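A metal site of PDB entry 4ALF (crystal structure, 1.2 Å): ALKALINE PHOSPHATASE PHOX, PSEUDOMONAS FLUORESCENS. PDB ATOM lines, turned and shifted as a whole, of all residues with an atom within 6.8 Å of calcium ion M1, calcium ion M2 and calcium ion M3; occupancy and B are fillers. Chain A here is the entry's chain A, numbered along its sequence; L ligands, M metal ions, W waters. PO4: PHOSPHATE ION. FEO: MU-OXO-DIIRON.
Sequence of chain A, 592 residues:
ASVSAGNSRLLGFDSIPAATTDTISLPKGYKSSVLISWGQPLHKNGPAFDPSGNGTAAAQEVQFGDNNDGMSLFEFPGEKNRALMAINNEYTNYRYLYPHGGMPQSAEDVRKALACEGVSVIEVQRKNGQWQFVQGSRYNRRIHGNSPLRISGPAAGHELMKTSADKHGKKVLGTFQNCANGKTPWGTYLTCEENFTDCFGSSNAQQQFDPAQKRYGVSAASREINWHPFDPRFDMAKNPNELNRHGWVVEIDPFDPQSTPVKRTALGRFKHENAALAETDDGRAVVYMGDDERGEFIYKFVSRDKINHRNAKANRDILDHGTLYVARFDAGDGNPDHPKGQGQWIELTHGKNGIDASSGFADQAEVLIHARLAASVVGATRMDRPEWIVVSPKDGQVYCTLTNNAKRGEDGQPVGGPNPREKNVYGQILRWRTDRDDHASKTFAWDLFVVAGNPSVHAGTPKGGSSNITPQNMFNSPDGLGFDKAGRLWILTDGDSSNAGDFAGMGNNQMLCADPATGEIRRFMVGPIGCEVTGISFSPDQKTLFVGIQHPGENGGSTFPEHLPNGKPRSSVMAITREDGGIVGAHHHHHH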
ATOM      1  N   ASP A  69     -20.120 -11.201 -11.518  1.00  0.00           N
ATOM      2  CA  ASP A  69     -18.928 -10.577 -12.074  1.00  0.00           C
ATOM      3  C   ASP A  69     -18.207  -9.842 -10.950  1.00  0.00           C
ATOM      4  O   ASP A  69     -17.884 -10.468  -9.929  1.00  0.00           O
ATOM      5  CB  ASP A  69     -19.345  -9.697 -13.284  1.00  0.00           C
ATOM      6  CG  ASP A  69     -18.236  -9.468 -14.286  1.00  0.00           C
ATOM      7  OD1 ASP A  69     -17.047  -9.532 -13.911  1.00  0.00           O
ATOM      8  OD2 ASP A  69     -18.597  -9.197 -15.447  1.00  0.00           O
ATOM      9  N   GLU A  90     -23.850  -9.332 -14.559  1.00  0.00           N
ATOM     10  CA  GLU A  90     -23.556  -8.606 -15.787  1.00  0.00           C
ATOM     11  C   GLU A  90     -24.572  -8.783 -16.915  1.00  0.00           C
ATOM     12  O   GLU A  90     -24.939  -7.813 -17.608  1.00  0.00           O
ATOM     13  CB  GLU A  90     -22.142  -8.954 -16.305  1.00  0.00           C
ATOM     14  CG  GLU A  90     -21.698  -8.031 -17.436  1.00  0.00           C
ATOM     15  CD  GLU A  90     -20.348  -8.394 -17.980  1.00  0.00           C
ATOM     16  OE1 GLU A  90     -20.087  -9.616 -18.164  1.00  0.00           O
ATOM     17  OE2 GLU A  90     -19.569  -7.448 -18.317  1.00  0.00           O
ATOM     18  N   TYR A  91     -24.986 -10.029 -17.159  1.00  0.00           N
ATOM     19  CA  TYR A  91     -25.857 -10.323 -18.292  1.00  0.00           C
ATOM     20  C   TYR A  91     -26.526 -11.650 -18.049  1.00  0.00           C
ATOM     21  O   TYR A  91     -26.388 -12.202 -16.950  1.00  0.00           O
ATOM     22  CB  TYR A  91     -25.107 -10.250 -19.642  1.00  0.00           C
ATOM     23  CG  TYR A  91     -24.042 -11.275 -19.951  1.00  0.00           C
ATOM     24  CD1 TYR A  91     -22.800 -11.209 -19.368  1.00  0.00           C
ATOM     25  CD2 TYR A  91     -24.236 -12.250 -20.938  1.00  0.00           C
ATOM     26  CE1 TYR A  91     -21.783 -12.071 -19.701  1.00  0.00           C
ATOM     27  CE2 TYR A  91     -23.221 -13.117 -21.295  1.00  0.00           C
ATOM     28  CZ  TYR A  91     -21.981 -13.058 -20.676  1.00  0.00           C
ATOM     29  OH  TYR A  91     -20.939 -13.897 -21.019  1.00  0.00           O
ATOM     30  N   CYS A 179     -20.444  -4.778 -14.922  1.00  0.00           N
ATOM     31  CA  CYS A 179     -19.236  -5.534 -15.171  1.00  0.00           C
ATOM     32  C   CYS A 179     -18.413  -5.655 -13.918  1.00  0.00           C
ATOM     33  O   CYS A 179     -18.646  -6.596 -13.151  1.00  0.00           O
ATOM     34  CB  CYS A 179     -18.487  -4.874 -16.323  1.00  0.00           C
ATOM     35  SG  CYS A 179     -16.987  -5.727 -16.806  1.00  0.00           S
ATOM     36  N   ALA A 180     -17.502  -4.730 -13.664  1.00  0.00           N
ATOM     37  CA  ALA A 180     -16.739  -4.812 -12.429  1.00  0.00           C
ATOM     38  C   ALA A 180     -16.931  -3.595 -11.529  1.00  0.00           C
ATOM     39  O   ALA A 180     -17.960  -2.915 -11.622  1.00  0.00           O
ATOM     40  CB  ALA A 180     -15.292  -5.211 -12.721  1.00  0.00           C
ATOM     41  N   GLU A 194     -20.843  -1.479 -18.520  1.00  0.00           N
ATOM     42  CA  GLU A 194     -19.918  -1.753 -19.631  1.00  0.00           C
ATOM     43  C   GLU A 194     -20.654  -1.839 -20.962  1.00  0.00           C
ATOM     44  O   GLU A 194     -20.781  -0.821 -21.642  1.00  0.00           O
ATOM     45  CB  GLU A 194     -19.032  -2.965 -19.347  1.00  0.00           C
ATOM     46  CG  GLU A 194     -17.968  -3.222 -20.374  1.00  0.00           C
ATOM     47  CD  GLU A 194     -17.386  -4.618 -20.260  1.00  0.00           C
ATOM     48  OE1 GLU A 194     -18.083  -5.532 -19.722  1.00  0.00           O
ATOM     49  OE2 GLU A 194     -16.259  -4.813 -20.735  1.00  0.00           O
ATOM     50  N   GLU A 273     -15.192  -0.827 -17.232  1.00  0.00           N
ATOM     51  CA  GLU A 273     -14.872  -2.143 -16.697  1.00  0.00           C
ATOM     52  C   GLU A 273     -14.889  -2.105 -15.154  1.00  0.00           C
ATOM     53  O   GLU A 273     -15.816  -2.624 -14.540  1.00  0.00           O
ATOM     54  CB  GLU A 273     -13.551  -2.679 -17.242  1.00  0.00           C
ATOM     55  CG  GLU A 273     -13.301  -4.091 -16.728  1.00  0.00           C
ATOM     56  CD  GLU A 273     -13.641  -5.196 -17.709  1.00  0.00           C
ATOM     57  OE1 GLU A 273     -13.906  -4.889 -18.907  1.00  0.00           O
ATOM     58  OE2 GLU A 273     -13.646  -6.367 -17.248  1.00  0.00           O
ATOM     59  N   ASP A 292     -13.472  -0.718 -21.951  1.00  0.00           N
ATOM     60  CA  ASP A 292     -13.168  -1.969 -22.637  1.00  0.00           C
ATOM     61  C   ASP A 292     -13.799  -2.028 -23.988  1.00  0.00           C
ATOM     62  O   ASP A 292     -14.910  -2.480 -24.167  1.00  0.00           O
ATOM     63  CB  ASP A 292     -13.545  -3.193 -21.822  1.00  0.00           C
ATOM     64  CG  ASP A 292     -13.242  -4.477 -22.564  1.00  0.00           C
ATOM     65  OD1 ASP A 292     -12.569  -4.422 -23.617  1.00  0.00           O
ATOM     66  OD2 ASP A 292     -13.668  -5.556 -22.077  1.00  0.00           O
ATOM     67  N   ARG A 385      -7.931  -3.067 -25.353  1.00  0.00           N
ATOM     68  CA  ARG A 385      -9.034  -3.503 -24.478  1.00  0.00           C
ATOM     69  C   ARG A 385      -8.678  -3.458 -23.013  1.00  0.00           C
ATOM     70  O   ARG A 385      -8.508  -4.509 -22.350  1.00  0.00           O
ATOM     71  CB  ARG A 385      -9.514  -4.903 -24.854  1.00  0.00           C
ATOM     72  CG  ARG A 385     -10.223  -4.969 -26.182  1.00  0.00           C
ATOM     73  CD  ARG A 385     -10.850  -6.323 -26.358  1.00  0.00           C
ATOM     74  NE  ARG A 385     -11.856  -6.514 -25.319  1.00  0.00           N
ATOM     75  CZ  ARG A 385     -12.413  -7.686 -25.010  1.00  0.00           C
ATOM     76  NH1 ARG A 385     -12.118  -8.782 -25.682  1.00  0.00           N
ATOM     77  NH2 ARG A 385     -13.279  -7.733 -24.019  1.00  0.00           N
ATOM     78  N   GLU A 387      -9.217  -3.727 -19.364  1.00  0.00           N
ATOM     79  CA  GLU A 387     -10.249  -4.289 -18.480  1.00  0.00           C
ATOM     80  C   GLU A 387      -9.912  -3.836 -17.045  1.00  0.00           C
ATOM     81  O   GLU A 387      -9.911  -2.634 -16.767  1.00  0.00           O
ATOM     82  CB  GLU A 387     -10.449  -5.799 -18.718  1.00  0.00           C
ATOM     83  CG  GLU A 387     -11.111  -6.043 -20.058  1.00  0.00           C
ATOM     84  CD  GLU A 387     -11.771  -7.387 -20.196  1.00  0.00           C
ATOM     85  OE1 GLU A 387     -11.030  -8.361 -20.393  1.00  0.00           O
ATOM     86  OE2 GLU A 387     -13.016  -7.519 -20.126  1.00  0.00           O
ATOM     87  N   TRP A 388      -9.641  -4.720 -16.101  1.00  0.00           N
ATOM     88  CA  TRP A 388      -9.520  -4.270 -14.727  1.00  0.00           C
ATOM     89  C   TRP A 388      -8.237  -3.546 -14.423  1.00  0.00           C
ATOM     90  O   TRP A 388      -7.184  -3.882 -14.965  1.00  0.00           O
ATOM     91  CB  TRP A 388      -9.594  -5.399 -13.712  1.00  0.00           C
ATOM     92  CG  TRP A 388     -10.899  -6.160 -13.673  1.00  0.00           C
ATOM     93  CD1 TRP A 388     -11.685  -6.556 -14.731  1.00  0.00           C
ATOM     94  CD2 TRP A 388     -11.517  -6.736 -12.496  1.00  0.00           C
ATOM     95  NE1 TRP A 388     -12.771  -7.305 -14.297  1.00  0.00           N
ATOM     96  CE2 TRP A 388     -12.685  -7.470 -12.976  1.00  0.00           C
ATOM     97  CE3 TRP A 388     -11.229  -6.740 -11.150  1.00  0.00           C
ATOM     98  CZ2 TRP A 388     -13.525  -8.150 -12.103  1.00  0.00           C
ATOM     99  CZ3 TRP A 388     -12.055  -7.458 -10.299  1.00  0.00           C
ATOM    100  CH2 TRP A 388     -13.176  -8.130 -10.757  1.00  0.00           C
ATOM    101  N   THR A 403      -6.661  -6.966 -22.523  1.00  0.00           N
ATOM    102  CA  THR A 403      -7.016  -8.395 -22.594  1.00  0.00           C
ATOM    103  C   THR A 403      -6.625  -9.071 -23.899  1.00  0.00           C
ATOM    104  O   THR A 403      -6.172 -10.211 -23.902  1.00  0.00           O
ATOM    105  CB  THR A 403      -8.486  -8.634 -22.191  1.00  0.00           C
ATOM    106  OG1 THR A 403      -8.661 -10.009 -21.850  1.00  0.00           O
ATOM    107  CG2 THR A 403      -9.476  -8.190 -23.227  1.00  0.00           C
ATOM    108  N   ASN A 404      -6.794  -8.348 -24.999  1.00  0.00           N
ATOM    109  CA  ASN A 404      -6.450  -8.763 -26.348  1.00  0.00           C
ATOM    110  C   ASN A 404      -6.871  -7.650 -27.302  1.00  0.00           C
ATOM    111  O   ASN A 404      -7.524  -6.672 -26.898  1.00  0.00           O
ATOM    112  CB  ASN A 404      -7.064 -10.120 -26.728  1.00  0.00           C
ATOM    113  CG  ASN A 404      -8.556 -10.186 -26.499  1.00  0.00           C
ATOM    114  OD1 ASN A 404      -9.335  -9.396 -27.038  1.00  0.00           O
ATOM    115  ND2 ASN A 404      -9.002 -11.162 -25.670  1.00  0.00           N
ATOM    116  N   SER A 477      -5.750 -13.812 -22.323  1.00  0.00           N
ATOM    117  CA  SER A 477      -6.839 -12.884 -22.042  1.00  0.00           C
ATOM    118  C   SER A 477      -7.016 -12.621 -20.562  1.00  0.00           C
ATOM    119  O   SER A 477      -8.122 -12.792 -20.036  1.00  0.00           O
ATOM    120  CB  SER A 477      -8.149 -13.340 -22.698  1.00  0.00           C
ATOM    121  OG  SER A 477      -7.986 -13.541 -24.111  1.00  0.00           O
ATOM    122  N   PRO A 478      -5.978 -12.162 -19.862  1.00  0.00           N
ATOM    123  CA  PRO A 478      -6.172 -11.719 -18.494  1.00  0.00           C
ATOM    124  C   PRO A 478      -7.215 -10.584 -18.490  1.00  0.00           C
ATOM    125  O   PRO A 478      -7.280  -9.803 -19.449  1.00  0.00           O
ATOM    126  CB  PRO A 478      -4.778 -11.205 -18.123  1.00  0.00           C
ATOM    127  CG  PRO A 478      -4.195 -10.709 -19.419  1.00  0.00           C
ATOM    128  CD  PRO A 478      -4.716 -11.677 -20.443  1.00  0.00           C
ATOM    129  N   ASP A 479      -8.044 -10.544 -17.460  1.00  0.00           N
ATOM    130  CA  ASP A 479      -9.220  -9.685 -17.414  1.00  0.00           C
ATOM    131  C   ASP A 479      -9.280  -9.122 -15.987  1.00  0.00           C
ATOM    132  O   ASP A 479      -8.786  -8.020 -15.726  1.00  0.00           O
ATOM    133  CB  ASP A 479     -10.432 -10.513 -17.889  1.00  0.00           C
ATOM    134  CG  ASP A 479     -11.783  -9.769 -17.880  1.00  0.00           C
ATOM    135  OD1 ASP A 479     -11.958  -8.828 -17.094  1.00  0.00           O
ATOM    136  OD2 ASP A 479     -12.662 -10.195 -18.650  1.00  0.00           O
ATOM    137  N   GLY A 480      -9.784  -9.913 -15.060  1.00  0.00           N
ATOM    138  CA  GLY A 480      -9.804  -9.500 -13.688  1.00  0.00           C
ATOM    139  C   GLY A 480      -8.477  -9.468 -12.977  1.00  0.00           C
ATOM    140  O   GLY A 480      -7.567 -10.205 -13.330  1.00  0.00           O
ATOM    141  N   THR A 493      -8.722 -14.961 -15.662  1.00  0.00           N
ATOM    142  CA  THR A 493      -8.767 -14.963 -17.118  1.00  0.00           C
ATOM    143  C   THR A 493     -10.161 -15.124 -17.726  1.00  0.00           C
ATOM    144  O   THR A 493     -11.043 -15.818 -17.219  1.00  0.00           O
ATOM    145  CB  THR A 493      -7.788 -15.996 -17.763  1.00  0.00           C
ATOM    146  OG1 THR A 493      -8.303 -17.339 -17.717  1.00  0.00           O
ATOM    147  CG2 THR A 493      -6.444 -15.961 -17.054  1.00  0.00           C
ATOM    148  N   ASP A 494     -10.318 -14.522 -18.889  1.00  0.00           N
ATOM    149  CA  ASP A 494     -11.528 -14.576 -19.689  1.00  0.00           C
ATOM    150  C   ASP A 494     -11.108 -14.723 -21.149  1.00  0.00           C
ATOM    151  O   ASP A 494     -11.271 -13.817 -21.958  1.00  0.00           O
ATOM    152  CB  ASP A 494     -12.372 -13.307 -19.540  1.00  0.00           C
ATOM    153  CG  ASP A 494     -13.553 -13.264 -20.463  1.00  0.00           C
ATOM    154  OD1 ASP A 494     -14.025 -14.338 -20.891  1.00  0.00           O
ATOM    155  OD2 ASP A 494     -14.049 -12.165 -20.813  1.00  0.00           O
ATOM    156  N   GLY A 495     -10.571 -15.875 -21.489  1.00  0.00           N
ATOM    157  CA  GLY A 495     -10.004 -16.098 -22.791  1.00  0.00           C
ATOM    158  C   GLY A 495     -10.599 -17.286 -23.471  1.00  0.00           C
ATOM    159  O   GLY A 495     -11.606 -17.861 -23.067  1.00  0.00           O
ATOM    160  N   GLU A 532     -15.946 -18.094 -17.522  1.00  0.00           N
ATOM    161  CA  GLU A 532     -14.782 -17.267 -17.267  1.00  0.00           C
ATOM    162  C   GLU A 532     -14.682 -17.122 -15.757  1.00  0.00           C
ATOM    163  O   GLU A 532     -15.664 -17.298 -15.024  1.00  0.00           O
ATOM    164  CB  GLU A 532     -14.831 -15.908 -17.981  1.00  0.00           C
ATOM    165  CG  GLU A 532     -15.940 -14.977 -17.524  1.00  0.00           C
ATOM    166  CD  GLU A 532     -16.089 -13.806 -18.481  1.00  0.00           C
ATOM    167  OE1 GLU A 532     -16.711 -13.992 -19.530  1.00  0.00           O
ATOM    168  OE2 GLU A 532     -15.524 -12.730 -18.185  1.00  0.00           O
ATOM    169  N   THR A 534     -14.029 -14.558 -12.787  1.00  0.00           N
ATOM    170  CA  THR A 534     -14.195 -13.102 -12.675  1.00  0.00           C
ATOM    171  C   THR A 534     -14.783 -12.784 -11.325  1.00  0.00           C
ATOM    172  O   THR A 534     -15.571 -13.548 -10.801  1.00  0.00           O
ATOM    173  CB  THR A 534     -15.031 -12.590 -13.859  1.00  0.00           C
ATOM    174  OG1 THR A 534     -14.998 -11.161 -13.857  1.00  0.00           O
ATOM    175  CG2 THR A 534     -16.458 -13.134 -13.846  1.00  0.00           C
ATOM    176  N   GLN A 550     -18.396 -17.369 -13.919  1.00  0.00           N
ATOM    177  CA  GLN A 550     -19.430 -16.731 -14.684  1.00  0.00           C
ATOM    178  C   GLN A 550     -19.750 -17.567 -15.939  1.00  0.00           C
ATOM    179  O   GLN A 550     -18.844 -18.088 -16.588  1.00  0.00           O
ATOM    180  CB  GLN A 550     -18.989 -15.309 -15.113  1.00  0.00           C
ATOM    181  CG  GLN A 550     -20.118 -14.465 -15.686  1.00  0.00           C
ATOM    182  CD  GLN A 550     -19.592 -13.219 -16.363  1.00  0.00           C
ATOM    183  OE1 GLN A 550     -18.713 -13.296 -17.217  1.00  0.00           O
ATOM    184  NE2 GLN A 550     -20.098 -12.059 -15.935  1.00  0.00           N
ATOM    185  N   HIS A 551     -21.049 -17.699 -16.221  1.00  0.00           N
ATOM    186  CA  HIS A 551     -21.598 -18.429 -17.381  1.00  0.00           C
ATOM    187  C   HIS A 551     -20.994 -19.788 -17.610  1.00  0.00           C
ATOM    188  O   HIS A 551     -20.654 -20.124 -18.745  1.00  0.00           O
ATOM    189  CB  HIS A 551     -21.586 -17.581 -18.688  1.00  0.00           C
ATOM    190  CG  HIS A 551     -20.228 -17.122 -19.148  1.00  0.00           C
ATOM    191  ND1 HIS A 551     -19.312 -17.943 -19.700  1.00  0.00           N
ATOM    192  CD2 HIS A 551     -19.686 -15.863 -19.156  1.00  0.00           C
ATOM    193  CE1 HIS A 551     -18.227 -17.235 -20.012  1.00  0.00           C
ATOM    194  NE2 HIS A 551     -18.445 -15.973 -19.664  1.00  0.00           N
HETATM  195  P   PO4 L   1     -16.232  -8.916 -21.012  1.00  0.00           P
HETATM  196  O1  PO4 L   1     -15.327  -9.648 -19.999  1.00  0.00           O
HETATM  197  O2  PO4 L   1     -17.558  -8.458 -20.380  1.00  0.00           O
HETATM  198  O3  PO4 L   1     -15.428  -7.825 -21.702  1.00  0.00           O
HETATM  199  O4  PO4 L   1     -16.604  -9.982 -22.028  1.00  0.00           O
HETATM  200 FE1  FEO L   2     -17.590  -7.269 -18.694  1.00  0.00          FE
HETATM  201 FE2  FEO L   2     -14.640  -6.207 -20.451  1.00  0.00          FE
HETATM  202  O   FEO L   2     -15.617  -7.056 -19.008  1.00  0.00           O
HETATM  203 CA    CA M   1     -13.067  -9.915 -20.888  1.00  0.00          CA
HETATM  204 CA    CA M   2     -14.355  -8.645 -17.780  1.00  0.00          CA
HETATM  205 CA    CA M   3     -16.434 -11.899 -20.626  1.00  0.00          CA
HETATM  206  O   HOH W   1     -18.028 -11.281 -18.985  1.00  0.00           O
HETATM  207  O   HOH W   2     -16.985  -9.078 -17.495  1.00  0.00           O
HETATM  208  O   HOH W   3     -18.639 -12.450 -21.695  1.00  0.00           O
HETATM  209  O   HOH W   4     -16.011 -13.335 -22.647  1.00  0.00           O
HETATM  210  O   HOH W   5     -11.230 -10.997 -21.836  1.00  0.00           O
HETATM  211  O   HOH W   6     -14.474 -10.826 -16.553  1.00  0.00           O
HETATM  212  O   HOH W   7     -14.103 -10.281 -23.154  1.00  0.00           O
HETATM  213  O   HOH W   8     -15.198  -8.089 -15.479  1.00  0.00           O
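FE2 of FEO L2 is bound by OE2 of Glu 387, 2.1 Å away.
SG of Cys 179 is bound to FE1 of FEO L2, 2.5 Å away.
The side-chain carboxylate of Glu 194 is bound to an iron atom (FE1) of FEO L2 (2.1 Å).
The side-chain carboxylate (OE1) of Glu 273 is bound to an iron atom (FE2) of FEO L2, at 2.2 Å.
An iron atom (FE1) of FEO L2 is bound by the side-chain carboxylate (OE2) of Glu 90, at 2.0 Å.
The side-chain carboxylate (OD2) of Asp 292 binds an iron atom (FE2) of FEO L2 (2.0 Å).
O of Arg 385 is in hydrogen-bond range of N of Thr 403 (3.1 Å).
OG1 of Thr 403 sits close to OE1 of Glu 387 (3.2 Å).
The guanidinium group (NE) of Arg 385 lies within salt-bridge range of the side-chain carboxylate (OD1) of Asp 292 (2.8 Å).
The backbone NH (N) of Asp 494 lies within hydrogen-bond range of the backbone carbonyl oxygen (O) of Ser 477 (3.0 Å).
The guanidinium group (NH1) of Arg 385 lies within hydrogen-bond range of the side-chain amide oxygen (OD1) of Asn 404.
O of Glu 273 sits at hydrogen-bond distance from N of Ala 180, 2.8 Å away.
OE2 of Glu 273 lies close to NE1 of Trp 388, 3.2 Å away.
The backbone carbonyl oxygen (O) of Asp 479 lies close to the backbone NH (N) of Trp 388.
NH2 of Arg 385 touches calcium ion M1 (3.8 Å).
Four residues have an atom within 4 Å of calcium ion M1: Arg 385, Glu 387, Asp 479 and Asp 494.
The nearest printed residue that does not touch calcium ion M1 is Thr 403 (4.5 Å).
Within 4 Å of calcium ion M3: Asp 494 and Glu 532.
The nearest printed residue that does not touch calcium ion M3 is Gln 550 (4.3 Å).
Calcium ion M1 is bound by the side-chain carboxylate (OD2) of Asp 479 (2.3 Å), water W5 (2.3 Å), an oxygen (O1) of PO4 L1 (2.4 Å), the side-chain carboxylate (OD2) of Asp 494 (2.5 Å), the side-chain carboxylate (OE2) of Glu 387 (2.5 Å), water W7 (2.5 Å) and the side-chain carboxylate (OE1) of Glu 387 (2.6 Å).
An oxygen (O) of FEO L2 binds calcium ion M2, at 2.4 Å.
Calcium ion M2 is bound by OE2 of Glu 273, at 2.4 Å.
OD2 of Asp 479 is bound to calcium ion M2, 2.5 Å away.
The side-chain carboxylate (OD1) of Asp 479 is bound to calcium ion M2 (2.5 Å).
Water W6 binds calcium ion M2, at 2.5 Å.
Water W8 is bound to calcium ion M2, at 2.5 Å.
Calcium ion M2 is bound by O1 of PO4 L1.
Water W2 is bound to calcium ion M2 (2.7 Å).
Calcium ion M2 has eight donor atoms within binding distance.
Slightly farther from calcium ion M2 lies the side-chain carboxylate (OE2) of Glu 387 (2.9 Å).
Calcium ion M3 is bound by water W1, 2.4 Å away.
OE1 of Glu 532 binds calcium ion M3 (2.4 Å).
O4 of PO4 L1 binds calcium ion M3, 2.4 Å away.
OD2 of Asp 494 binds calcium ion M3.
Calcium ion M3 is bound by water W3 (2.5 Å).
Calcium ion M3 is bound by water W4, at 2.5 Å.
An oxygen (O1) of PO4 L1 binds calcium ion M3 (2.6 Å).
OE2 of Glu 532 is bound to calcium ion M3, at 2.7 Å.
Calcium ion M3 has eight donor atoms within binding distance.
Water W5 lies within hydrogen-bond range of the side-chain hydroxyl (OG1) of Thr 403 (2.8 Å) and the backbone carbonyl oxygen (O) of Asp 494 (2.8 Å).
Water W8 lies within hydrogen-bond range of the indole nitrogen (NE1) of Trp 388 (2.8 Å), the side-chain carboxylate (OD1) of Asp 69 (2.8 Å) and the side-chain hydroxyl (OG1) of Thr 534 (3.5 Å).
Water W2 lies within hydrogen-bond range of the side-chain carboxylate of Asp 69 (2.6 Å) and the side-chain carboxylate of Glu 90 (3.2 Å).
Water W1 lies within hydrogen-bond range of OE1 of Gln 550 (2.8 Å) and OE1 of Glu 90 (2.8 Å).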
